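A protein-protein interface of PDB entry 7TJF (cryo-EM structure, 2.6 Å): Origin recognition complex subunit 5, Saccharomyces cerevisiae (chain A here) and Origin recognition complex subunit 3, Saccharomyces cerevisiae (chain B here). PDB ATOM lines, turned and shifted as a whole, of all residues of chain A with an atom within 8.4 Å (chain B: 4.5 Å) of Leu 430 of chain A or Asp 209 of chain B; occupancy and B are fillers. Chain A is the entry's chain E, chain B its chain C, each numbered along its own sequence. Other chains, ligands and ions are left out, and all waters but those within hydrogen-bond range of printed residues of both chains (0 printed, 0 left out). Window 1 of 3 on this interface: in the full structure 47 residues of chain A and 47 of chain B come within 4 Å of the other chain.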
ATOM      1  N   ASP A 323       5.640  -2.964   7.363  1.00  0.00           N
ATOM      2  CA  ASP A 323       6.074  -3.380   8.691  1.00  0.00           C
ATOM      3  C   ASP A 323       6.420  -4.860   8.738  1.00  0.00           C
ATOM      4  O   ASP A 323       5.912  -5.597   9.582  1.00  0.00           O
ATOM      5  CB  ASP A 323       4.999  -3.071   9.733  1.00  0.00           C
ATOM      6  CG  ASP A 323       4.856  -1.592  10.001  1.00  0.00           C
ATOM      7  OD1 ASP A 323       4.307  -0.879   9.136  1.00  0.00           O
ATOM      8  OD2 ASP A 323       5.286  -1.142  11.084  1.00  0.00           O
ATOM      9  N   LEU A 324       7.292  -5.291   7.837  1.00  0.00           N
ATOM     10  CA  LEU A 324       7.842  -6.635   7.863  1.00  0.00           C
ATOM     11  C   LEU A 324       9.300  -6.574   8.295  1.00  0.00           C
ATOM     12  O   LEU A 324       9.943  -5.523   8.245  1.00  0.00           O
ATOM     13  CB  LEU A 324       7.739  -7.311   6.493  1.00  0.00           C
ATOM     14  CG  LEU A 324       6.355  -7.701   5.980  1.00  0.00           C
ATOM     15  CD1 LEU A 324       6.470  -8.294   4.585  1.00  0.00           C
ATOM     16  CD2 LEU A 324       5.667  -8.670   6.926  1.00  0.00           C
ATOM     17  N   SER A 328      12.007 -11.248   6.436  1.00  0.00           N
ATOM     18  CA  SER A 328      10.737 -11.453   5.742  1.00  0.00           C
ATOM     19  C   SER A 328      10.709 -10.729   4.399  1.00  0.00           C
ATOM     20  O   SER A 328      10.196 -11.265   3.408  1.00  0.00           O
ATOM     21  CB  SER A 328       9.573 -10.987   6.618  1.00  0.00           C
ATOM     22  OG  SER A 328       9.366 -11.864   7.709  1.00  0.00           O
ATOM     23  N   LEU A 332      10.497 -12.594   0.825  1.00  0.00           N
ATOM     24  CA  LEU A 332       9.485 -12.255  -0.174  1.00  0.00           C
ATOM     25  C   LEU A 332      10.112 -11.947  -1.531  1.00  0.00           C
ATOM     26  O   LEU A 332       9.596 -12.379  -2.572  1.00  0.00           O
ATOM     27  CB  LEU A 332       8.654 -11.069   0.306  1.00  0.00           C
ATOM     28  CG  LEU A 332       7.222 -11.366   0.736  1.00  0.00           C
ATOM     29  CD1 LEU A 332       6.561 -10.110   1.269  1.00  0.00           C
ATOM     30  CD2 LEU A 332       6.436 -11.932  -0.428  1.00  0.00           C
ATOM     31  N   ASN A 423      10.250 -16.748  10.086  1.00  0.00           N
ATOM     32  CA  ASN A 423       9.808 -15.679   9.195  1.00  0.00           C
ATOM     33  C   ASN A 423       9.083 -16.235   7.976  1.00  0.00           C
ATOM     34  O   ASN A 423       8.087 -15.660   7.528  1.00  0.00           O
ATOM     35  CB  ASN A 423      11.008 -14.834   8.764  1.00  0.00           C
ATOM     36  CG  ASN A 423      11.355 -13.757   9.770  1.00  0.00           C
ATOM     37  OD1 ASN A 423      10.513 -12.943  10.141  1.00  0.00           O
ATOM     38  ND2 ASN A 423      12.597 -13.761  10.234  1.00  0.00           N
ATOM     39  N   LEU A 424       9.572 -17.353   7.432  1.00  0.00           N
ATOM     40  CA  LEU A 424       8.916 -17.997   6.298  1.00  0.00           C
ATOM     41  C   LEU A 424       7.533 -18.528   6.674  1.00  0.00           C
ATOM     42  O   LEU A 424       6.577 -18.399   5.900  1.00  0.00           O
ATOM     43  CB  LEU A 424       9.806 -19.125   5.777  1.00  0.00           C
ATOM     44  CG  LEU A 424       9.424 -19.866   4.497  1.00  0.00           C
ATOM     45  CD1 LEU A 424       8.949 -18.906   3.413  1.00  0.00           C
ATOM     46  CD2 LEU A 424      10.609 -20.680   4.020  1.00  0.00           C
ATOM     47  N   SER A 425       7.412 -19.122   7.865  1.00  0.00           N
ATOM     48  CA  SER A 425       6.118 -19.605   8.341  1.00  0.00           C
ATOM     49  C   SER A 425       5.157 -18.451   8.608  1.00  0.00           C
ATOM     50  O   SER A 425       3.949 -18.570   8.368  1.00  0.00           O
ATOM     51  CB  SER A 425       6.315 -20.456   9.596  1.00  0.00           C
ATOM     52  OG  SER A 425       5.154 -21.205   9.907  1.00  0.00           O
ATOM     53  N   GLU A 426       5.679 -17.327   9.111  1.00  0.00           N
ATOM     54  CA  GLU A 426       4.863 -16.125   9.280  1.00  0.00           C
ATOM     55  C   GLU A 426       4.400 -15.573   7.937  1.00  0.00           C
ATOM     56  O   GLU A 426       3.268 -15.091   7.813  1.00  0.00           O
ATOM     57  CB  GLU A 426       5.650 -15.068  10.061  1.00  0.00           C
ATOM     58  CG  GLU A 426       4.904 -13.754  10.342  1.00  0.00           C
ATOM     59  CD  GLU A 426       3.984 -13.793  11.561  1.00  0.00           C
ATOM     60  OE1 GLU A 426       3.508 -14.878  11.956  1.00  0.00           O
ATOM     61  OE2 GLU A 426       3.732 -12.711  12.130  1.00  0.00           O
ATOM     62  N   LEU A 427       5.266 -15.624   6.921  1.00  0.00           N
ATOM     63  CA  LEU A 427       4.869 -15.216   5.577  1.00  0.00           C
ATOM     64  C   LEU A 427       3.815 -16.149   4.992  1.00  0.00           C
ATOM     65  O   LEU A 427       2.964 -15.707   4.212  1.00  0.00           O
ATOM     66  CB  LEU A 427       6.085 -15.164   4.652  1.00  0.00           C
ATOM     67  CG  LEU A 427       7.089 -14.021   4.792  1.00  0.00           C
ATOM     68  CD1 LEU A 427       8.213 -14.199   3.787  1.00  0.00           C
ATOM     69  CD2 LEU A 427       6.420 -12.673   4.621  1.00  0.00           C
ATOM     70  N   HIS A 428       3.859 -17.435   5.343  1.00  0.00           N
ATOM     71  CA  HIS A 428       2.822 -18.343   4.863  1.00  0.00           C
ATOM     72  C   HIS A 428       1.494 -18.113   5.577  1.00  0.00           C
ATOM     73  O   HIS A 428       0.431 -18.184   4.949  1.00  0.00           O
ATOM     74  CB  HIS A 428       3.245 -19.798   5.019  1.00  0.00           C
ATOM     75  CG  HIS A 428       2.201 -20.766   4.558  1.00  0.00           C
ATOM     76  ND1 HIS A 428       1.446 -21.521   5.429  1.00  0.00           N
ATOM     77  CD2 HIS A 428       1.764 -21.078   3.316  1.00  0.00           C
ATOM     78  CE1 HIS A 428       0.600 -22.267   4.742  1.00  0.00           C
ATOM     79  NE2 HIS A 428       0.774 -22.018   3.458  1.00  0.00           N
ATOM     80  N   THR A 429       1.522 -17.843   6.884  1.00  0.00           N
ATOM     81  CA  THR A 429       0.266 -17.616   7.590  1.00  0.00           C
ATOM     82  C   THR A 429      -0.332 -16.241   7.307  1.00  0.00           C
ATOM     83  O   THR A 429      -1.503 -16.016   7.627  1.00  0.00           O
ATOM     84  CB  THR A 429       0.437 -17.816   9.104  1.00  0.00           C
ATOM     85  OG1 THR A 429      -0.851 -17.979   9.708  1.00  0.00           O
ATOM     86  CG2 THR A 429       1.123 -16.633   9.751  1.00  0.00           C
ATOM     87  N   LEU A 430       0.429 -15.328   6.712  1.00  0.00           N
ATOM     88  CA  LEU A 430      -0.115 -14.070   6.225  1.00  0.00           C
ATOM     89  C   LEU A 430      -0.582 -14.159   4.780  1.00  0.00           C
ATOM     90  O   LEU A 430      -1.171 -13.194   4.282  1.00  0.00           O
ATOM     91  CB  LEU A 430       0.927 -12.956   6.367  1.00  0.00           C
ATOM     92  CG  LEU A 430       1.187 -12.464   7.792  1.00  0.00           C
ATOM     93  CD1 LEU A 430       2.200 -11.335   7.797  1.00  0.00           C
ATOM     94  CD2 LEU A 430      -0.112 -12.027   8.454  1.00  0.00           C
ATOM     95  N   LYS A 431      -0.351 -15.304   4.123  1.00  0.00           N
ATOM     96  CA  LYS A 431      -0.620 -15.519   2.695  1.00  0.00           C
ATOM     97  C   LYS A 431       0.010 -14.457   1.796  1.00  0.00           C
ATOM     98  O   LYS A 431      -0.625 -13.913   0.892  1.00  0.00           O
ATOM     99  CB  LYS A 431      -2.113 -15.698   2.410  1.00  0.00           C
ATOM    100  CG  LYS A 431      -2.718 -16.878   3.155  1.00  0.00           C
ATOM    101  CD  LYS A 431      -4.037 -16.651   3.843  1.00  0.00           C
ATOM    102  CE  LYS A 431      -4.419 -17.963   4.518  1.00  0.00           C
ATOM    103  NZ  LYS A 431      -5.085 -17.857   5.832  1.00  0.00           N
ATOM    104  N   LEU A 432       1.286 -14.174   2.051  1.00  0.00           N
ATOM    105  CA  LEU A 432       2.164 -13.598   1.045  1.00  0.00           C
ATOM    106  C   LEU A 432       2.947 -14.667   0.298  1.00  0.00           C
ATOM    107  O   LEU A 432       3.475 -14.391  -0.783  1.00  0.00           O
ATOM    108  CB  LEU A 432       3.125 -12.597   1.691  1.00  0.00           C
ATOM    109  CG  LEU A 432       2.434 -11.601   2.626  1.00  0.00           C
ATOM    110  CD1 LEU A 432       3.445 -10.721   3.343  1.00  0.00           C
ATOM    111  CD2 LEU A 432       1.422 -10.758   1.866  1.00  0.00           C
ATOM    112  N   ILE A 433       3.033 -15.868   0.869  1.00  0.00           N
ATOM    113  CA  ILE A 433       3.458 -17.091   0.200  1.00  0.00           C
ATOM    114  C   ILE A 433       2.280 -18.054   0.250  1.00  0.00           C
ATOM    115  O   ILE A 433       1.505 -18.053   1.211  1.00  0.00           O
ATOM    116  CB  ILE A 433       4.709 -17.718   0.867  1.00  0.00           C
ATOM    117  CG1 ILE A 433       5.704 -16.637   1.291  1.00  0.00           C
ATOM    118  CG2 ILE A 433       5.393 -18.731  -0.047  1.00  0.00           C
ATOM    119  CD1 ILE A 433       6.359 -15.920   0.148  1.00  0.00           C
ATOM    120  N   ALA A 434       2.136 -18.871  -0.789  1.00  0.00           N
ATOM    121  CA  ALA A 434       1.066 -19.851  -0.854  1.00  0.00           C
ATOM    122  C   ALA A 434       1.634 -21.217  -1.213  1.00  0.00           C
ATOM    123  O   ALA A 434       2.765 -21.342  -1.693  1.00  0.00           O
ATOM    124  CB  ALA A 434      -0.015 -19.446  -1.868  1.00  0.00           C
ATOM    125  N   ASN A 453       2.750 -14.878  -3.587  1.00  0.00           N
ATOM    126  CA  ASN A 453       1.340 -14.500  -3.563  1.00  0.00           C
ATOM    127  C   ASN A 453       1.181 -12.991  -3.429  1.00  0.00           C
ATOM    128  O   ASN A 453       0.246 -12.504  -2.786  1.00  0.00           O
ATOM    129  CB  ASN A 453       0.594 -15.221  -2.438  1.00  0.00           C
ATOM    130  CG  ASN A 453      -0.872 -15.455  -2.766  1.00  0.00           C
ATOM    131  OD1 ASN A 453      -1.233 -15.713  -3.915  1.00  0.00           O
ATOM    132  ND2 ASN A 453      -1.725 -15.354  -1.756  1.00  0.00           N
ATOM    133  N   VAL A 454       2.085 -12.229  -4.037  1.00  0.00           N
ATOM    134  CA  VAL A 454       1.977 -10.772  -4.054  1.00  0.00           C
ATOM    135  C   VAL A 454       2.093 -10.296  -5.499  1.00  0.00           C
ATOM    136  O   VAL A 454       2.737 -10.968  -6.316  1.00  0.00           O
ATOM    137  CB  VAL A 454       3.043 -10.113  -3.158  1.00  0.00           C
ATOM    138  CG1 VAL A 454       2.720 -10.325  -1.685  1.00  0.00           C
ATOM    139  CG2 VAL A 454       4.428 -10.634  -3.489  1.00  0.00           C
ATOM    140  N   ASP B 207      -7.547 -11.379  12.371  1.00  0.00           N
ATOM    141  CA  ASP B 207      -6.630 -11.915  11.352  1.00  0.00           C
ATOM    142  C   ASP B 207      -7.182 -11.734   9.935  1.00  0.00           C
ATOM    143  O   ASP B 207      -7.431 -12.703   9.215  1.00  0.00           O
ATOM    144  CB  ASP B 207      -6.276 -13.381  11.630  1.00  0.00           C
ATOM    145  CG  ASP B 207      -6.030 -13.652  13.101  1.00  0.00           C
ATOM    146  OD1 ASP B 207      -5.021 -13.147  13.637  1.00  0.00           O
ATOM    147  OD2 ASP B 207      -6.842 -14.368  13.726  1.00  0.00           O
ATOM    148  N   VAL B 208      -7.392 -10.467   9.553  1.00  0.00           N
ATOM    149  CA  VAL B 208      -8.012 -10.102   8.276  1.00  0.00           C
ATOM    150  C   VAL B 208      -7.158 -10.565   7.092  1.00  0.00           C
ATOM    151  O   VAL B 208      -7.683 -10.902   6.022  1.00  0.00           O
ATOM    152  CB  VAL B 208      -8.283  -8.576   8.278  1.00  0.00           C
ATOM    153  CG1 VAL B 208      -8.613  -8.015   6.891  1.00  0.00           C
ATOM    154  CG2 VAL B 208      -9.388  -8.246   9.260  1.00  0.00           C
ATOM    155  N   ASP B 209      -5.849 -10.703   7.290  1.00  0.00           N
ATOM    156  CA  ASP B 209      -4.978 -11.256   6.261  1.00  0.00           C
ATOM    157  C   ASP B 209      -5.176 -12.753   6.038  1.00  0.00           C
ATOM    158  O   ASP B 209      -4.551 -13.313   5.130  1.00  0.00           O
ATOM    159  CB  ASP B 209      -3.515 -10.995   6.624  1.00  0.00           C
ATOM    160  CG  ASP B 209      -3.075  -9.596   6.274  1.00  0.00           C
ATOM    161  OD1 ASP B 209      -3.110  -9.246   5.076  1.00  0.00           O
ATOM    162  OD2 ASP B 209      -2.695  -8.845   7.195  1.00  0.00           O
ATOM    163  N   SER B 210      -6.013 -13.414   6.839  1.00  0.00           N
ATOM    164  CA  SER B 210      -6.262 -14.837   6.705  1.00  0.00           C
ATOM    165  C   SER B 210      -7.660 -15.182   6.205  1.00  0.00           C
ATOM    166  O   SER B 210      -7.849 -16.281   5.677  1.00  0.00           O
ATOM    167  CB  SER B 210      -6.024 -15.538   8.049  1.00  0.00           C
ATOM    168  OG  SER B 210      -4.887 -15.004   8.703  1.00  0.00           O
ATOM    169  N   ILE B 211      -8.636 -14.283   6.352  1.00  0.00           N
ATOM    170  CA  ILE B 211      -9.987 -14.562   5.879  1.00  0.00           C
ATOM    171  C   ILE B 211     -10.017 -14.431   4.360  1.00  0.00           C
ATOM    172  O   ILE B 211      -9.329 -13.579   3.779  1.00  0.00           O
ATOM    173  CB  ILE B 211     -11.001 -13.630   6.577  1.00  0.00           C
ATOM    174  CG1 ILE B 211     -12.418 -13.773   6.018  1.00  0.00           C
ATOM    175  CG2 ILE B 211     -10.607 -12.181   6.463  1.00  0.00           C
ATOM    176  CD1 ILE B 211     -13.476 -13.348   6.979  1.00  0.00           C
ATOM    177  N   ILE B 240      -5.575  -5.601  10.815  1.00  0.00           N
ATOM    178  CA  ILE B 240      -4.693  -5.666   9.657  1.00  0.00           C
ATOM    179  C   ILE B 240      -3.288  -5.982  10.144  1.00  0.00           C
ATOM    180  O   ILE B 240      -2.770  -5.313  11.047  1.00  0.00           O
ATOM    181  CB  ILE B 240      -4.710  -4.335   8.886  1.00  0.00           C
ATOM    182  CG1 ILE B 240      -6.145  -3.876   8.617  1.00  0.00           C
ATOM    183  CG2 ILE B 240      -3.929  -4.456   7.588  1.00  0.00           C
ATOM    184  CD1 ILE B 240      -6.945  -4.832   7.795  1.00  0.00           C
ATOM    185  N   ASN B 241      -2.660  -6.993   9.551  1.00  0.00           N
ATOM    186  CA  ASN B 241      -1.306  -7.353   9.945  1.00  0.00           C
ATOM    187  C   ASN B 241      -0.240  -6.905   8.955  1.00  0.00           C
ATOM    188  O   ASN B 241       0.886  -6.625   9.372  1.00  0.00           O
ATOM    189  CB  ASN B 241      -1.193  -8.868  10.149  1.00  0.00           C
ATOM    190  CG  ASN B 241      -0.492  -9.230  11.443  1.00  0.00           C
ATOM    191  OD1 ASN B 241      -0.217  -8.367  12.275  1.00  0.00           O
ATOM    192  ND2 ASN B 241      -0.196 -10.511  11.617  1.00  0.00           N
ATOM    193  N   THR B 242      -0.557  -6.813   7.662  1.00  0.00           N
ATOM    194  CA  THR B 242       0.481  -6.559   6.654  1.00  0.00           C
ATOM    195  C   THR B 242       0.617  -5.067   6.352  1.00  0.00           C
ATOM    196  O   THR B 242       1.624  -4.451   6.709  1.00  0.00           O
ATOM    197  CB  THR B 242       0.171  -7.357   5.386  1.00  0.00           C
ATOM    198  OG1 THR B 242      -0.016  -8.736   5.724  1.00  0.00           O
ATOM    199  CG2 THR B 242       1.316  -7.255   4.398  1.00  0.00           C
ATOM    200  N   ILE B 247      -4.707  -4.786   1.578  1.00  0.00           N
ATOM    201  CA  ILE B 247      -6.101  -5.110   1.849  1.00  0.00           C
ATOM    202  C   ILE B 247      -7.004  -4.562   0.751  1.00  0.00           C
ATOM    203  O   ILE B 247      -7.898  -5.263   0.260  1.00  0.00           O
ATOM    204  CB  ILE B 247      -6.493  -4.577   3.242  1.00  0.00           C
ATOM    205  CG1 ILE B 247      -5.674  -5.265   4.342  1.00  0.00           C
ATOM    206  CG2 ILE B 247      -7.978  -4.762   3.506  1.00  0.00           C
ATOM    207  CD1 ILE B 247      -5.515  -6.770   4.197  1.00  0.00           C
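Of the printed residues of chain B, Leu 430 of chain A touches Asp 209 (3.5 Å), Asn 241 (3.5 Å) and Thr 242 (3.995 Å). Printed residues of chain A within 4 Å of Asp 209 of chain B: Leu 430 and Lys 431. Of the printed residues of chain B, Lys 431 of chain A touches Asp 209 and Ser 210. Of the printed residues of chain A, Asn 241 of chain B touches Leu 430 (3.5 Å). Printed residues of chain A within 4 Å of Thr 242 of chain B: Leu 430 (3.995 Å). Ser 425 of chain A touches none of the printed residues of chain B.
Among the printed residues, merely in contact across the chains: Thr 429 of chain A with Ser 210 of chain B, Leu 430 of chain A with Asn 241 of chain B, Leu 430 of chain A with Thr 242 of chain B and Lys 431 of chain A with Asp 209 of chain B.
The side-chain amino group (NZ) of Lys 431 of chain A sits at hydrogen-bond distance from the backbone carbonyl oxygen (O) of Ser 210 of chain B, at 3.2 Å. The backbone carbonyl oxygen (O) of Leu 430 of chain A lies close to the backbone carbonyl oxygen (O) of Asp 209 of chain B (3.5 Å).
The backbone carbonyl oxygen (O) of Asp 207 of chain B sits close to the side-chain hydroxyl (OG) of Ser 210 of chain B, at 3.5 Å. The side-chain carboxylate (OD2) of Asp 209 of chain B is in hydrogen-bond range of the backbone NH (N) of Asn 241 of chain B, 3.0 Å away. The side-chain carboxylate of Asp 209 of chain B is in hydrogen-bond range of the backbone NH of Thr 242 of chain B, 3.0 Å away. The side-chain amide nitrogen (ND2) of Asn 453 of chain A is in hydrogen-bond range of the backbone carbonyl oxygen (O) of Lys 431 of chain A (3.2 Å).
Of the 9 printed residues of chain B, 4 touch a printed residue of chain A. Of the 18 printed residues of chain A, 3 touch a printed residue of chain B. Printed residues of chain A that touch a printed residue of chain B: Thr 429, Leu 430 and Lys 431. Hydrophobic or aromatic side chains of chain A within 4 Å of the printed part of chain B: Leu 430. Among the printed residues, 6 pairs touch across the chains. Among the printed residues, no Asp or Glu carboxylate lies within 4 Å of a Lys or Arg side-chain nitrogen of the other chain.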
